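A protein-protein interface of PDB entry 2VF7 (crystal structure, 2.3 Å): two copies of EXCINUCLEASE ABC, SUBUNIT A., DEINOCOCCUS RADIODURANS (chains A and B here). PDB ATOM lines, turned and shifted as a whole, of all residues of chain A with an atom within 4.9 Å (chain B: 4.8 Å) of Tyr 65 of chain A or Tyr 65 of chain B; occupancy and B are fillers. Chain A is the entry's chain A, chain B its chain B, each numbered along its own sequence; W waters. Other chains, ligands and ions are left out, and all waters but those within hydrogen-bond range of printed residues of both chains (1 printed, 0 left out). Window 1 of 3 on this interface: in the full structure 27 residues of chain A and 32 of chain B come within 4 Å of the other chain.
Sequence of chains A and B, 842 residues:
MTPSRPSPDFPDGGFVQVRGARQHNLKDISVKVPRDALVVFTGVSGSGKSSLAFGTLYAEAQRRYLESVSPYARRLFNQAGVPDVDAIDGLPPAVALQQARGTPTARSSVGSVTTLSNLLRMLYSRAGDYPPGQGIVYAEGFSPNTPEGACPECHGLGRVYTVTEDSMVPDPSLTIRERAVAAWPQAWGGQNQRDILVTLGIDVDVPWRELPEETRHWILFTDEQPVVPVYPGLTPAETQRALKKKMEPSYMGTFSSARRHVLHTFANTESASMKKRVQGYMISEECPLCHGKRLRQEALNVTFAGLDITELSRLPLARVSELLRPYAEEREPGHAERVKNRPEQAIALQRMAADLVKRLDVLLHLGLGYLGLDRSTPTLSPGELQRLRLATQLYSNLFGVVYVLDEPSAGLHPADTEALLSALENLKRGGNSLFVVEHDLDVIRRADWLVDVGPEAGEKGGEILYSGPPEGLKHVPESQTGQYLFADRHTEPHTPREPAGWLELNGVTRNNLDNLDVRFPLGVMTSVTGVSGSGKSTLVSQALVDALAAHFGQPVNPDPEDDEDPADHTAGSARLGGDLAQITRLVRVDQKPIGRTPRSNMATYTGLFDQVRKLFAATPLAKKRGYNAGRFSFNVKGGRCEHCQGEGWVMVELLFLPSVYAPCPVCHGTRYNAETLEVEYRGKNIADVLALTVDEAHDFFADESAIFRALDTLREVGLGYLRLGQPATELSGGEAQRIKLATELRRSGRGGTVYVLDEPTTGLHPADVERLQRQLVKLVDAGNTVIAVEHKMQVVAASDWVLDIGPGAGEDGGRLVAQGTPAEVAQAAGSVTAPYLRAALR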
ATOM      1  N   ALA A  61     -32.825 -36.826  28.529  1.00  0.00           N
ATOM      2  CA  ALA A  61     -32.810 -35.433  28.067  1.00  0.00           C
ATOM      3  C   ALA A  61     -31.565 -35.033  27.272  1.00  0.00           C
ATOM      4  O   ALA A  61     -31.669 -34.237  26.337  1.00  0.00           O
ATOM      5  CB  ALA A  61     -33.007 -34.487  29.234  1.00  0.00           C
ATOM      6  N   GLN A  62     -30.396 -35.558  27.646  1.00  0.00           N
ATOM      7  CA  GLN A  62     -29.140 -35.250  26.930  1.00  0.00           C
ATOM      8  C   GLN A  62     -28.939 -36.031  25.659  1.00  0.00           C
ATOM      9  O   GLN A  62     -28.491 -35.480  24.663  1.00  0.00           O
ATOM     10  CB  GLN A  62     -27.908 -35.433  27.814  1.00  0.00           C
ATOM     11  CG  GLN A  62     -27.522 -34.174  28.559  1.00  0.00           C
ATOM     12  CD  GLN A  62     -26.025 -33.868  28.515  1.00  0.00           C
ATOM     13  OE1 GLN A  62     -25.624 -32.699  28.669  1.00  0.00           O
ATOM     14  NE2 GLN A  62     -25.193 -34.903  28.307  1.00  0.00           N
ATOM     15  N   ARG A  63     -29.232 -37.325  25.701  1.00  0.00           N
ATOM     16  CA  ARG A  63     -29.255 -38.156  24.502  1.00  0.00           C
ATOM     17  C   ARG A  63     -30.089 -37.538  23.367  1.00  0.00           C
ATOM     18  O   ARG A  63     -29.655 -37.518  22.228  1.00  0.00           O
ATOM     19  CB  ARG A  63     -29.810 -39.537  24.866  1.00  0.00           C
ATOM     20  CG  ARG A  63     -29.914 -40.524  23.718  1.00  0.00           C
ATOM     21  CD  ARG A  63     -31.018 -41.517  24.021  1.00  0.00           C
ATOM     22  NE  ARG A  63     -31.493 -42.185  22.818  1.00  0.00           N
ATOM     23  CZ  ARG A  63     -32.713 -42.042  22.302  1.00  0.00           C
ATOM     24  NH1 ARG A  63     -33.617 -41.251  22.888  1.00  0.00           N
ATOM     25  NH2 ARG A  63     -33.036 -42.707  21.197  1.00  0.00           N
ATOM     26  N   ARG A  64     -31.286 -37.061  23.689  1.00  0.00           N
ATOM     27  CA  ARG A  64     -32.221 -36.505  22.703  1.00  0.00           C
ATOM     28  C   ARG A  64     -31.679 -35.247  22.044  1.00  0.00           C
ATOM     29  O   ARG A  64     -31.701 -35.116  20.817  1.00  0.00           O
ATOM     30  CB  ARG A  64     -33.558 -36.166  23.362  1.00  0.00           C
ATOM     31  CG  ARG A  64     -34.366 -37.365  23.764  1.00  0.00           C
ATOM     32  CD  ARG A  64     -35.681 -36.942  24.371  1.00  0.00           C
ATOM     33  NE  ARG A  64     -36.517 -38.101  24.636  1.00  0.00           N
ATOM     34  CZ  ARG A  64     -37.647 -38.050  25.327  1.00  0.00           C
ATOM     35  NH1 ARG A  64     -38.077 -36.885  25.810  1.00  0.00           N
ATOM     36  NH2 ARG A  64     -38.351 -39.159  25.532  1.00  0.00           N
ATOM     37  N   TYR A  65     -31.203 -34.326  22.878  1.00  0.00           N
ATOM     38  CA  TYR A  65     -30.646 -33.072  22.400  1.00  0.00           C
ATOM     39  C   TYR A  65     -29.476 -33.303  21.452  1.00  0.00           C
ATOM     40  O   TYR A  65     -29.496 -32.811  20.313  1.00  0.00           O
ATOM     41  CB  TYR A  65     -30.281 -32.130  23.568  1.00  0.00           C
ATOM     42  CG  TYR A  65     -29.912 -30.732  23.113  1.00  0.00           C
ATOM     43  CD1 TYR A  65     -30.893 -29.814  22.715  1.00  0.00           C
ATOM     44  CD2 TYR A  65     -28.575 -30.338  23.040  1.00  0.00           C
ATOM     45  CE1 TYR A  65     -30.544 -28.537  22.274  1.00  0.00           C
ATOM     46  CE2 TYR A  65     -28.219 -29.068  22.593  1.00  0.00           C
ATOM     47  CZ  TYR A  65     -29.206 -28.177  22.221  1.00  0.00           C
ATOM     48  OH  TYR A  65     -28.825 -26.924  21.802  1.00  0.00           O
ATOM     49  N   LEU A  66     -28.481 -34.072  21.896  1.00  0.00           N
ATOM     50  CA  LEU A  66     -27.254 -34.264  21.106  1.00  0.00           C
ATOM     51  C   LEU A  66     -27.464 -35.009  19.795  1.00  0.00           C
ATOM     52  O   LEU A  66     -26.713 -34.814  18.853  1.00  0.00           O
ATOM     53  CB  LEU A  66     -26.151 -34.930  21.933  1.00  0.00           C
ATOM     54  CG  LEU A  66     -25.588 -34.140  23.117  1.00  0.00           C
ATOM     55  CD1 LEU A  66     -24.967 -35.101  24.138  1.00  0.00           C
ATOM     56  CD2 LEU A  66     -24.580 -33.074  22.681  1.00  0.00           C
ATOM     57  N   GLU A  67     -28.479 -35.863  19.740  1.00  0.00           N
ATOM     58  CA  GLU A  67     -28.835 -36.566  18.508  1.00  0.00           C
ATOM     59  C   GLU A  67     -29.587 -35.665  17.523  1.00  0.00           C
ATOM     60  O   GLU A  67     -29.684 -35.960  16.335  1.00  0.00           O
ATOM     61  CB  GLU A  67     -29.701 -37.769  18.828  1.00  0.00           C
ATOM     62  CG  GLU A  67     -28.999 -38.907  19.542  1.00  0.00           C
ATOM     63  CD  GLU A  67     -29.834 -40.175  19.527  1.00  0.00           C
ATOM     64  OE1 GLU A  67     -30.843 -40.225  18.775  1.00  0.00           O
ATOM     65  OE2 GLU A  67     -29.486 -41.123  20.262  1.00  0.00           O
ATOM     66  N   SER A  68     -30.137 -34.578  18.029  1.00  0.00           N
ATOM     67  CA  SER A  68     -30.780 -33.595  17.196  1.00  0.00           C
ATOM     68  C   SER A  68     -29.787 -32.578  16.677  1.00  0.00           C
ATOM     69  O   SER A  68     -29.927 -32.121  15.542  1.00  0.00           O
ATOM     70  CB  SER A  68     -31.880 -32.897  17.972  1.00  0.00           C
ATOM     71  OG  SER A  68     -32.945 -33.792  18.192  1.00  0.00           O
ATOM     72  N   VAL A  69     -28.788 -32.214  17.483  1.00  0.00           N
ATOM     73  CA  VAL A  69     -27.763 -31.272  17.014  1.00  0.00           C
ATOM     74  C   VAL A  69     -26.695 -31.951  16.147  1.00  0.00           C
ATOM     75  O   VAL A  69     -26.179 -31.340  15.199  1.00  0.00           O
ATOM     76  CB  VAL A  69     -27.141 -30.398  18.144  1.00  0.00           C
ATOM     77  CG1 VAL A  69     -28.229 -29.663  18.911  1.00  0.00           C
ATOM     78  CG2 VAL A  69     -26.285 -31.209  19.084  1.00  0.00           C
ATOM     79  N   PRO A  93     -34.237 -29.553  27.615  1.00  0.00           N
ATOM     80  CA  PRO A  93     -32.830 -29.979  27.711  1.00  0.00           C
ATOM     81  C   PRO A  93     -32.297 -29.863  29.145  1.00  0.00           C
ATOM     82  O   PRO A  93     -32.890 -29.155  29.955  1.00  0.00           O
ATOM     83  CB  PRO A  93     -32.113 -29.012  26.765  1.00  0.00           C
ATOM     84  CG  PRO A  93     -33.196 -28.556  25.813  1.00  0.00           C
ATOM     85  CD  PRO A  93     -34.400 -28.411  26.697  1.00  0.00           C
ATOM     86  N   ALA A  94     -31.202 -30.567  29.454  1.00  0.00           N
ATOM     87  CA  ALA A  94     -30.704 -30.654  30.822  1.00  0.00           C
ATOM     88  C   ALA A  94     -29.203 -30.408  30.955  1.00  0.00           C
ATOM     89  O   ALA A  94     -28.424 -30.844  30.113  1.00  0.00           O
ATOM     90  CB  ALA A  94     -31.072 -32.011  31.429  1.00  0.00           C
ATOM     91  N   VAL A  95     -28.820 -29.740  32.048  1.00  0.00           N
ATOM     92  CA  VAL A  95     -27.427 -29.529  32.459  1.00  0.00           C
ATOM     93  C   VAL A  95     -27.199 -30.170  33.841  1.00  0.00           C
ATOM     94  O   VAL A  95     -27.933 -29.884  34.771  1.00  0.00           O
ATOM     95  CB  VAL A  95     -27.098 -28.005  32.545  1.00  0.00           C
ATOM     96  CG1 VAL A  95     -25.613 -27.783  32.778  1.00  0.00           C
ATOM     97  CG2 VAL A  95     -27.554 -27.274  31.274  1.00  0.00           C
ATOM     98  N   LEU A 398     -28.677 -18.498  30.665  1.00  0.00           N
ATOM     99  CA  LEU A 398     -29.420 -19.691  30.204  1.00  0.00           C
ATOM    100  C   LEU A 398     -30.875 -19.682  30.661  1.00  0.00           C
ATOM    101  O   LEU A 398     -31.162 -19.357  31.822  1.00  0.00           O
ATOM    102  CB  LEU A 398     -28.784 -20.997  30.686  1.00  0.00           C
ATOM    103  CG  LEU A 398     -27.918 -21.813  29.739  1.00  0.00           C
ATOM    104  CD1 LEU A 398     -28.061 -23.306  30.052  1.00  0.00           C
ATOM    105  CD2 LEU A 398     -28.292 -21.545  28.296  1.00  0.00           C
ATOM    106  N   VAL A 401     -33.855 -24.557  30.690  1.00  0.00           N
ATOM    107  CA  VAL A 401     -33.184 -25.865  30.841  1.00  0.00           C
ATOM    108  C   VAL A 401     -33.578 -26.426  32.218  1.00  0.00           C
ATOM    109  O   VAL A 401     -34.151 -25.697  33.025  1.00  0.00           O
ATOM    110  CB  VAL A 401     -31.602 -25.796  30.702  1.00  0.00           C
ATOM    111  CG1 VAL A 401     -31.166 -25.433  29.310  1.00  0.00           C
ATOM    112  CG2 VAL A 401     -30.971 -24.854  31.720  1.00  0.00           C
ATOM    113  N   ALA B  61     -27.166 -19.317  21.694  1.00  0.00           N
ATOM    114  CA  ALA B  61     -27.828 -20.429  22.380  1.00  0.00           C
ATOM    115  C   ALA B  61     -26.868 -21.601  22.496  1.00  0.00           C
ATOM    116  O   ALA B  61     -26.745 -22.208  23.556  1.00  0.00           O
ATOM    117  CB  ALA B  61     -29.076 -20.837  21.642  1.00  0.00           C
ATOM    118  N   GLN B  62     -26.185 -21.884  21.387  1.00  0.00           N
ATOM    119  CA  GLN B  62     -25.189 -22.940  21.267  1.00  0.00           C
ATOM    120  C   GLN B  62     -23.954 -22.730  22.132  1.00  0.00           C
ATOM    121  O   GLN B  62     -23.507 -23.660  22.802  1.00  0.00           O
ATOM    122  CB  GLN B  62     -24.763 -23.051  19.812  1.00  0.00           C
ATOM    123  CG  GLN B  62     -25.577 -24.046  19.015  1.00  0.00           C
ATOM    124  CD  GLN B  62     -24.833 -25.353  18.804  1.00  0.00           C
ATOM    125  OE1 GLN B  62     -25.376 -26.447  19.052  1.00  0.00           O
ATOM    126  NE2 GLN B  62     -23.571 -25.248  18.351  1.00  0.00           N
ATOM    127  N   ARG B  63     -23.391 -21.523  22.109  1.00  0.00           N
ATOM    128  CA  ARG B  63     -22.223 -21.230  22.930  1.00  0.00           C
ATOM    129  C   ARG B  63     -22.522 -21.402  24.417  1.00  0.00           C
ATOM    130  O   ARG B  63     -21.722 -21.985  25.141  1.00  0.00           O
ATOM    131  CB  ARG B  63     -21.705 -19.812  22.676  1.00  0.00           C
ATOM    132  CG  ARG B  63     -20.204 -19.679  22.829  1.00  0.00           C
ATOM    133  CD  ARG B  63     -19.792 -18.270  23.184  1.00  0.00           C
ATOM    134  NE  ARG B  63     -20.141 -17.946  24.568  1.00  0.00           N
ATOM    135  CZ  ARG B  63     -21.135 -17.136  24.929  1.00  0.00           C
ATOM    136  NH1 ARG B  63     -21.880 -16.548  24.003  1.00  0.00           N
ATOM    137  NH2 ARG B  63     -21.380 -16.909  26.214  1.00  0.00           N
ATOM    138  N   ARG B  64     -23.675 -20.894  24.853  1.00  0.00           N
ATOM    139  CA  ARG B  64     -24.059 -20.847  26.268  1.00  0.00           C
ATOM    140  C   ARG B  64     -24.404 -22.200  26.869  1.00  0.00           C
ATOM    141  O   ARG B  64     -24.334 -22.383  28.083  1.00  0.00           O
ATOM    142  CB  ARG B  64     -25.274 -19.960  26.451  1.00  0.00           C
ATOM    143  CG  ARG B  64     -25.044 -18.500  26.281  1.00  0.00           C
ATOM    144  CD  ARG B  64     -26.388 -17.869  26.329  1.00  0.00           C
ATOM    145  NE  ARG B  64     -26.333 -16.443  26.589  1.00  0.00           N
ATOM    146  CZ  ARG B  64     -27.380 -15.637  26.456  1.00  0.00           C
ATOM    147  NH1 ARG B  64     -28.555 -16.128  26.061  1.00  0.00           N
ATOM    148  NH2 ARG B  64     -27.257 -14.342  26.711  1.00  0.00           N
ATOM    149  N   TYR B  65     -24.827 -23.127  26.023  1.00  0.00           N
ATOM    150  CA  TYR B  65     -25.164 -24.451  26.461  1.00  0.00           C
ATOM    151  C   TYR B  65     -23.889 -25.271  26.559  1.00  0.00           C
ATOM    152  O   TYR B  65     -23.623 -25.878  27.601  1.00  0.00           O
ATOM    153  CB  TYR B  65     -26.154 -25.083  25.491  1.00  0.00           C
ATOM    154  CG  TYR B  65     -26.553 -26.505  25.819  1.00  0.00           C
ATOM    155  CD1 TYR B  65     -27.521 -26.768  26.782  1.00  0.00           C
ATOM    156  CD2 TYR B  65     -25.963 -27.587  25.162  1.00  0.00           C
ATOM    157  CE1 TYR B  65     -27.895 -28.073  27.093  1.00  0.00           C
ATOM    158  CE2 TYR B  65     -26.327 -28.911  25.470  1.00  0.00           C
ATOM    159  CZ  TYR B  65     -27.298 -29.137  26.429  1.00  0.00           C
ATOM    160  OH  TYR B  65     -27.686 -30.424  26.728  1.00  0.00           O
ATOM    161  N   LEU B  66     -23.102 -25.275  25.479  1.00  0.00           N
ATOM    162  CA  LEU B  66     -21.847 -26.037  25.415  1.00  0.00           C
ATOM    163  C   LEU B  66     -20.848 -25.672  26.520  1.00  0.00           C
ATOM    164  O   LEU B  66     -20.128 -26.541  27.011  1.00  0.00           O
ATOM    165  CB  LEU B  66     -21.177 -25.892  24.041  1.00  0.00           C
ATOM    166  CG  LEU B  66     -21.954 -26.167  22.748  1.00  0.00           C
ATOM    167  CD1 LEU B  66     -20.999 -26.104  21.548  1.00  0.00           C
ATOM    168  CD2 LEU B  66     -22.719 -27.494  22.771  1.00  0.00           C
ATOM    169  N   GLU B  67     -20.813 -24.391  26.897  1.00  0.00           N
ATOM    170  CA  GLU B  67     -19.992 -23.902  28.008  1.00  0.00           C
ATOM    171  C   GLU B  67     -20.516 -24.357  29.357  1.00  0.00           C
ATOM    172  O   GLU B  67     -19.778 -24.369  30.336  1.00  0.00           O
ATOM    173  CB  GLU B  67     -19.959 -22.379  28.023  1.00  0.00           C
ATOM    174  CG  GLU B  67     -19.095 -21.749  26.967  1.00  0.00           C
ATOM    175  CD  GLU B  67     -18.936 -20.253  27.173  1.00  0.00           C
ATOM    176  OE1 GLU B  67     -19.044 -19.794  28.334  1.00  0.00           O
ATOM    177  OE2 GLU B  67     -18.699 -19.535  26.176  1.00  0.00           O
ATOM    178  N   SER B  68     -21.804 -24.684  29.417  1.00  0.00           N
ATOM    179  CA  SER B  68     -22.456 -25.028  30.682  1.00  0.00           C
ATOM    180  C   SER B  68     -22.408 -26.527  30.911  1.00  0.00           C
ATOM    181  O   SER B  68     -22.333 -26.987  32.053  1.00  0.00           O
ATOM    182  CB  SER B  68     -23.903 -24.531  30.698  1.00  0.00           C
ATOM    183  OG  SER B  68     -23.948 -23.125  30.509  1.00  0.00           O
ATOM    184  N   VAL B  69     -22.458 -27.274  29.807  1.00  0.00           N
ATOM    185  CA  VAL B  69     -22.369 -28.725  29.825  1.00  0.00           C
ATOM    186  C   VAL B  69     -20.935 -29.185  30.075  1.00  0.00           C
ATOM    187  O   VAL B  69     -20.720 -30.074  30.897  1.00  0.00           O
ATOM    188  CB  VAL B  69     -22.935 -29.341  28.536  1.00  0.00           C
ATOM    189  CG1 VAL B  69     -22.285 -30.686  28.247  1.00  0.00           C
ATOM    190  CG2 VAL B  69     -24.453 -29.473  28.645  1.00  0.00           C
ATOM    191  N   PRO B  93     -32.463 -23.316  24.453  1.00  0.00           N
ATOM    192  CA  PRO B  93     -31.604 -24.120  23.571  1.00  0.00           C
ATOM    193  C   PRO B  93     -32.090 -24.159  22.105  1.00  0.00           C
ATOM    194  O   PRO B  93     -33.291 -24.153  21.846  1.00  0.00           O
ATOM    195  CB  PRO B  93     -31.667 -25.515  24.196  1.00  0.00           C
ATOM    196  CG  PRO B  93     -32.011 -25.282  25.615  1.00  0.00           C
ATOM    197  CD  PRO B  93     -32.855 -24.051  25.671  1.00  0.00           C
ATOM    198  N   ALA B  94     -31.145 -24.202  21.164  1.00  0.00           N
ATOM    199  CA  ALA B  94     -31.450 -24.084  19.734  1.00  0.00           C
ATOM    200  C   ALA B  94     -31.079 -25.345  18.988  1.00  0.00           C
ATOM    201  O   ALA B  94     -30.076 -25.961  19.319  1.00  0.00           O
ATOM    202  CB  ALA B  94     -30.692 -22.901  19.129  1.00  0.00           C
ATOM    203  N   VAL B  95     -31.891 -25.702  17.983  1.00  0.00           N
ATOM    204  CA  VAL B  95     -31.569 -26.767  17.010  1.00  0.00           C
ATOM    205  C   VAL B  95     -31.622 -26.217  15.553  1.00  0.00           C
ATOM    206  O   VAL B  95     -32.647 -25.688  15.125  1.00  0.00           O
ATOM    207  CB  VAL B  95     -32.505 -28.023  17.170  1.00  0.00           C
ATOM    208  CG1 VAL B  95     -32.124 -29.148  16.202  1.00  0.00           C
ATOM    209  CG2 VAL B  95     -32.468 -28.563  18.599  1.00  0.00           C
ATOM    210  N   LEU B 398     -38.358 -33.845  21.494  1.00  0.00           N
ATOM    211  CA  LEU B 398     -37.754 -32.621  21.999  1.00  0.00           C
ATOM    212  C   LEU B 398     -38.798 -31.633  22.473  1.00  0.00           C
ATOM    213  O   LEU B 398     -39.790 -31.382  21.797  1.00  0.00           O
ATOM    214  CB  LEU B 398     -36.858 -31.974  20.954  1.00  0.00           C
ATOM    215  CG  LEU B 398     -35.431 -32.521  20.912  1.00  0.00           C
ATOM    216  CD1 LEU B 398     -34.635 -31.772  19.881  1.00  0.00           C
ATOM    217  CD2 LEU B 398     -34.759 -32.397  22.274  1.00  0.00           C
ATOM    218  N   VAL B 401     -37.289 -26.365  22.894  1.00  0.00           N
ATOM    219  CA  VAL B 401     -36.173 -25.854  22.067  1.00  0.00           C
ATOM    220  C   VAL B 401     -36.653 -24.836  21.031  1.00  0.00           C
ATOM    221  O   VAL B 401     -37.852 -24.749  20.784  1.00  0.00           O
ATOM    222  CB  VAL B 401     -35.318 -27.001  21.396  1.00  0.00           C
ATOM    223  CG1 VAL B 401     -34.702 -27.886  22.447  1.00  0.00           C
ATOM    224  CG2 VAL B 401     -36.135 -27.831  20.429  1.00  0.00           C
HETATM  225  O   HOH W   1     -28.467 -24.432  22.729  1.00  0.00           O
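The side-chain hydroxyl (OH) of Tyr 65 of chain B sits at hydrogen-bond distance from the backbone carbonyl oxygen (O) of Ala 94 of chain A, at 3.5 Å.
OH of Tyr 65 of chain A sits at hydrogen-bond distance from O of Ala 94 of chain B (2.9 Å).
The backbone carbonyl oxygen (O) of Arg 64 of chain A lies within hydrogen-bond range of the side-chain hydroxyl (OG) of Ser 68 of chain A, at 3.2 Å.
The backbone carbonyl oxygen of Arg 64 of chain B sits at hydrogen-bond distance from the side-chain hydroxyl of Ser 68 of chain B, 2.6 Å away.
Among the printed residues, pairs that only touch across the chains: Gln 62 of chain A with Tyr 65 of chain B (3.6 Å), Gln 62 of chain A with Val 69 of chain B (3.4 Å), Tyr 65 of chain A with Tyr 65 of chain B (3.4 Å), Tyr 65 of chain A with Pro 93 of chain B (3.8 Å), Ser 68 of chain A with Val 95 of chain B (3.8 Å), Ser 68 of chain A with Leu 398 of chain B (3.1 Å), Pro 93 of chain A with Pro 93 of chain B (3.5 Å), Pro 93 of chain A with Val 401 of chain B (3.7 Å), Val 95 of chain A with Ser 68 of chain B (3.5 Å), Leu 398 of chain A with Arg 64 of chain B (3.9 Å) and Val 401 of chain A with Pro 93 of chain B (3.8 Å).
Of chain B, only Tyr 65 (3.4 Å), Pro 93 (3.8 Å) and Ala 94 (2.9 Å) come within 4 Å of Tyr 65 of chain A.
Printed residues of chain B within 4 Å of Ser 68 of chain A: Val 95 and Leu 398.
Printed residues of chain B within 4 Å of Val 401 of chain A: Pro 93 (3.8 Å).
Tyr 65 of chain B touches just these residues of chain A: Gln 62, Tyr 65 and Ala 94.
Of the printed residues of chain A, Pro 93 of chain B touches Tyr 65, Pro 93 and Val 401.
Printed residues of chain A within 4 Å of Leu 398 of chain B: Ser 68 (3.1 Å).
The nearest residue of chain A that does not touch Tyr 65 of chain B is Val 95 of chain A (4.3 Å).
The nearest printed residue of chain A that does not touch Val 401 of chain B is Tyr 65 of chain A (4.2 Å).
Of the 14 printed residues of chain A, 8 touch a printed residue of chain B.
Along chain A the printed residues that touch a printed residue of chain B span positions 62 to 401.
Printed residues of chain B that touch a printed residue of chain A: Arg 64, Tyr 65, Ser 68, Val 69, Pro 93, Ala 94, Val 95, Leu 398 and Val 401.
Gln 62 of chain A touches Tyr 65 of chain B, but with the chains exchanged Tyr 65 of chain A does not touch Gln 62 of chain B (4.4 Å).
Tyr 65 of chain A touches Pro 93 of chain B, but with the chains exchanged Pro 93 of chain A does not touch Tyr 65 of chain B (4.3 Å).
Tyr 65 of chain A touches Ala 94 of chain B, and with the chains exchanged Ala 94 of chain A touches Tyr 65 of chain B.
Pro 93 of chain A touches its own counterpart, Pro 93 of chain B.
14 positions are printed for both chains.
Water W1 lies within hydrogen-bond range of OH of Tyr 65 of chain A (2.7 Å), O of Ala 61 of chain B (2.9 Å) and N of Ala 94 of chain B (3.1 Å).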
